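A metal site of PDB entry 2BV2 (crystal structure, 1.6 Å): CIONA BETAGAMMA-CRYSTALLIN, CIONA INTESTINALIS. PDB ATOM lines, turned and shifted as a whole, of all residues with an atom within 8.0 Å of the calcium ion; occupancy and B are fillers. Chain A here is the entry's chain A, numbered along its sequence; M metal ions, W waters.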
ATOM      1  N   PHE A   6     -10.984  10.641 -25.662  1.00  0.00           N
ATOM      2  CA  PHE A   6     -10.053   9.550 -25.930  1.00  0.00           C
ATOM      3  C   PHE A   6      -8.697  10.065 -26.319  1.00  0.00           C
ATOM      4  O   PHE A   6      -8.593  11.001 -27.111  1.00  0.00           O
ATOM      5  CB  PHE A   6     -10.560   8.673 -27.084  1.00  0.00           C
ATOM      6  CG  PHE A   6     -11.779   7.864 -26.742  1.00  0.00           C
ATOM      7  CD1 PHE A   6     -11.664   6.559 -26.286  1.00  0.00           C
ATOM      8  CD2 PHE A   6     -13.040   8.409 -26.899  1.00  0.00           C
ATOM      9  CE1 PHE A   6     -12.810   5.815 -25.959  1.00  0.00           C
ATOM     10  CE2 PHE A   6     -14.189   7.675 -26.549  1.00  0.00           C
ATOM     11  CZ  PHE A   6     -14.077   6.400 -26.107  1.00  0.00           C
ATOM     12  N   GLU A   7      -7.657   9.382 -25.839  1.00  0.00           N
ATOM     13  CA  GLU A   7      -6.271   9.737 -26.125  1.00  0.00           C
ATOM     14  C   GLU A   7      -5.890   9.561 -27.594  1.00  0.00           C
ATOM     15  O   GLU A   7      -5.153  10.395 -28.146  1.00  0.00           O
ATOM     16  CB  GLU A   7      -5.375   8.874 -25.229  1.00  0.00           C
ATOM     17  CG  GLU A   7      -3.865   8.991 -25.459  1.00  0.00           C
ATOM     18  CD  GLU A   7      -3.146   7.683 -25.204  1.00  0.00           C
ATOM     19  OE1 GLU A   7      -3.814   6.701 -24.873  1.00  0.00           O
ATOM     20  OE2 GLU A   7      -1.906   7.625 -25.354  1.00  0.00           O
ATOM     21  N   ASP A   8      -6.382   8.483 -28.196  1.00  0.00           N
ATOM     22  CA  ASP A   8      -6.080   8.160 -29.592  1.00  0.00           C
ATOM     23  C   ASP A   8      -7.305   8.317 -30.503  1.00  0.00           C
ATOM     24  O   ASP A   8      -8.433   8.260 -30.065  1.00  0.00           O
ATOM     25  CB  ASP A   8      -5.587   6.715 -29.719  1.00  0.00           C
ATOM     26  CG  ASP A   8      -4.332   6.433 -28.877  1.00  0.00           C
ATOM     27  OD1 ASP A   8      -3.627   7.398 -28.474  1.00  0.00           O
ATOM     28  OD2 ASP A   8      -4.081   5.227 -28.613  1.00  0.00           O
ATOM     29  N   VAL A   9      -7.030   8.456 -31.794  1.00  0.00           N
ATOM     30  CA  VAL A   9      -8.062   8.423 -32.814  1.00  0.00           C
ATOM     31  C   VAL A   9      -8.846   7.109 -32.784  1.00  0.00           C
ATOM     32  O   VAL A   9      -8.403   6.082 -32.226  1.00  0.00           O
ATOM     33  CB  VAL A   9      -7.494   8.681 -34.247  1.00  0.00           C
ATOM     34  CG1 VAL A   9      -6.809  10.010 -34.316  1.00  0.00           C
ATOM     35  CG2 VAL A   9      -6.586   7.557 -34.684  1.00  0.00           C
ATOM     36  N   GLY A  12      -9.533   4.876 -29.402  1.00  0.00           N
ATOM     37  CA  GLY A  12      -8.500   4.086 -28.762  1.00  0.00           C
ATOM     38  C   GLY A  12      -7.814   4.794 -27.606  1.00  0.00           C
ATOM     39  O   GLY A  12      -8.030   5.993 -27.330  1.00  0.00           O
ATOM     40  N   ASP A  32      -4.136  18.402 -23.679  1.00  0.00           N
ATOM     41  CA  ASP A  32      -3.372  18.310 -24.918  1.00  0.00           C
ATOM     42  C   ASP A  32      -3.025  16.887 -25.341  1.00  0.00           C
ATOM     43  O   ASP A  32      -1.932  16.630 -25.851  1.00  0.00           O
ATOM     44  CB  ASP A  32      -2.131  19.189 -24.869  1.00  0.00           C
ATOM     45  CG  ASP A  32      -2.463  20.666 -24.802  1.00  0.00           C
ATOM     46  OD1 ASP A  32      -3.631  21.030 -24.990  1.00  0.00           O
ATOM     47  OD2 ASP A  32      -1.543  21.476 -24.568  1.00  0.00           O
ATOM     48  N   ILE A  33      -3.963  15.963 -25.125  1.00  0.00           N
ATOM     49  CA  ILE A  33      -3.814  14.613 -25.654  1.00  0.00           C
ATOM     50  C   ILE A  33      -5.002  14.073 -26.420  1.00  0.00           C
ATOM     51  O   ILE A  33      -4.873  13.016 -27.011  1.00  0.00           O
ATOM     52  CB  ILE A  33      -3.499  13.567 -24.546  1.00  0.00           C
ATOM     53  CG1 ILE A  33      -4.656  13.406 -23.569  1.00  0.00           C
ATOM     54  CG2 ILE A  33      -2.223  13.942 -23.810  1.00  0.00           C
ATOM     55  CD1 ILE A  33      -4.446  12.235 -22.627  1.00  0.00           C
ATOM     56  N   VAL A  34      -6.143  14.753 -26.413  1.00  0.00           N
ATOM     57  CA  VAL A  34      -7.360  14.176 -26.986  1.00  0.00           C
ATOM     58  C   VAL A  34      -7.303  14.125 -28.516  1.00  0.00           C
ATOM     59  O   VAL A  34      -6.955  15.109 -29.181  1.00  0.00           O
ATOM     60  CB  VAL A  34      -8.617  14.924 -26.525  1.00  0.00           C
ATOM     61  CG1 VAL A  34      -9.860  14.516 -27.367  1.00  0.00           C
ATOM     62  CG2 VAL A  34      -8.871  14.677 -25.044  1.00  0.00           C
ATOM     63  N   SER A  35      -7.633  12.953 -29.062  1.00  0.00           N
ATOM     64  CA  SER A  35      -7.609  12.719 -30.491  1.00  0.00           C
ATOM     65  C   SER A  35      -8.936  12.156 -31.051  1.00  0.00           C
ATOM     66  O   SER A  35      -9.104  12.111 -32.250  1.00  0.00           O
ATOM     67  CB  SER A  35      -6.434  11.813 -30.821  1.00  0.00           C
ATOM     68  OG  SER A  35      -5.190  12.411 -30.483  1.00  0.00           O
ATOM     69  N   SER A  36      -9.842  11.666 -30.193  1.00  0.00           N
ATOM     70  CA  SER A  36     -11.212  11.372 -30.608  1.00  0.00           C
ATOM     71  C   SER A  36     -12.172  11.548 -29.425  1.00  0.00           C
ATOM     72  O   SER A  36     -11.743  11.624 -28.262  1.00  0.00           O
ATOM     73  CB  SER A  36     -11.319   9.948 -31.168  1.00  0.00           C
ATOM     74  OG  SER A  36     -10.995   8.972 -30.198  1.00  0.00           O
ATOM     75  N   PRO A  67      -9.781  14.563 -34.782  1.00  0.00           N
ATOM     76  CA  PRO A  67     -10.055  15.981 -34.531  1.00  0.00           C
ATOM     77  C   PRO A  67     -10.696  16.725 -35.735  1.00  0.00           C
ATOM     78  O   PRO A  67     -11.546  17.620 -35.540  1.00  0.00           O
ATOM     79  CB  PRO A  67      -8.675  16.551 -34.162  1.00  0.00           C
ATOM     80  CG  PRO A  67      -7.852  15.368 -33.755  1.00  0.00           C
ATOM     81  CD  PRO A  67      -8.348  14.237 -34.622  1.00  0.00           C
ATOM     82  N   ASP A  74      -5.295  18.120 -33.355  1.00  0.00           N
ATOM     83  CA  ASP A  74      -4.945  16.978 -32.519  1.00  0.00           C
ATOM     84  C   ASP A  74      -4.207  17.456 -31.293  1.00  0.00           C
ATOM     85  O   ASP A  74      -3.425  18.387 -31.387  1.00  0.00           O
ATOM     86  CB  ASP A  74      -4.062  15.997 -33.290  1.00  0.00           C
ATOM     87  CG  ASP A  74      -3.865  14.706 -32.540  1.00  0.00           C
ATOM     88  OD1 ASP A  74      -4.859  14.168 -32.062  1.00  0.00           O
ATOM     89  OD2 ASP A  74      -2.703  14.260 -32.401  1.00  0.00           O
ATOM     90  N   ASP A  75      -4.476  16.813 -30.147  1.00  0.00           N
ATOM     91  CA  ASP A  75      -3.661  17.033 -28.956  1.00  0.00           C
ATOM     92  C   ASP A  75      -3.677  18.506 -28.517  1.00  0.00           C
ATOM     93  O   ASP A  75      -2.619  19.074 -28.202  1.00  0.00           O
ATOM     94  CB  ASP A  75      -2.211  16.558 -29.174  1.00  0.00           C
ATOM     95  CG  ASP A  75      -2.018  15.081 -28.905  1.00  0.00           C
ATOM     96  OD1 ASP A  75      -3.022  14.347 -28.863  1.00  0.00           O
ATOM     97  OD2 ASP A  75      -0.837  14.655 -28.704  1.00  0.00           O
ATOM     98  N   GLU A  76      -4.869  19.092 -28.493  1.00  0.00           N
ATOM     99  CA  GLU A  76      -5.056  20.495 -28.151  1.00  0.00           C
ATOM    100  C   GLU A  76      -6.213  20.830 -27.212  1.00  0.00           C
ATOM    101  O   GLU A  76      -6.284  21.939 -26.690  1.00  0.00           O
ATOM    102  CB  GLU A  76      -5.199  21.347 -29.414  1.00  0.00           C
ATOM    103  CG  GLU A  76      -4.838  22.814 -29.234  1.00  0.00           C
ATOM    104  CD  GLU A  76      -3.486  23.000 -28.607  1.00  0.00           C
ATOM    105  OE1 GLU A  76      -3.388  23.670 -27.540  1.00  0.00           O
ATOM    106  OE2 GLU A  76      -2.523  22.430 -29.185  1.00  0.00           O
HETATM  107 CA    CA M   1      -3.592  11.960 -28.778  1.00  0.00          CA
HETATM  108  O   HOH W   1      -2.063  12.225 -30.524  1.00  0.00           O
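N of Ser 35 lies within hydrogen-bond range of O of Phe 6. The backbone NH of Asp 75 sits at hydrogen-bond distance from the backbone carbonyl oxygen of Val 34.
Four residues have an atom within 4 Å of the calcium ion: Glu 7, Ile 33, Ser 35 and Asp 75.
The calcium ion is bound by the backbone carbonyl oxygen of Glu 7 (2.3 Å), water W1 (2.3 Å), the side-chain hydroxyl of Ser 35 (2.4 Å), the backbone carbonyl oxygen of Ile 33 (2.4 Å) and the side-chain carboxylate of Asp 75 (2.5 Å). The calcium ion has five donor atoms within binding distance.
Water W1 lies within hydrogen-bond range of the side-chain carboxylate of Asp 74 and the side-chain carboxylate of Asp 75.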
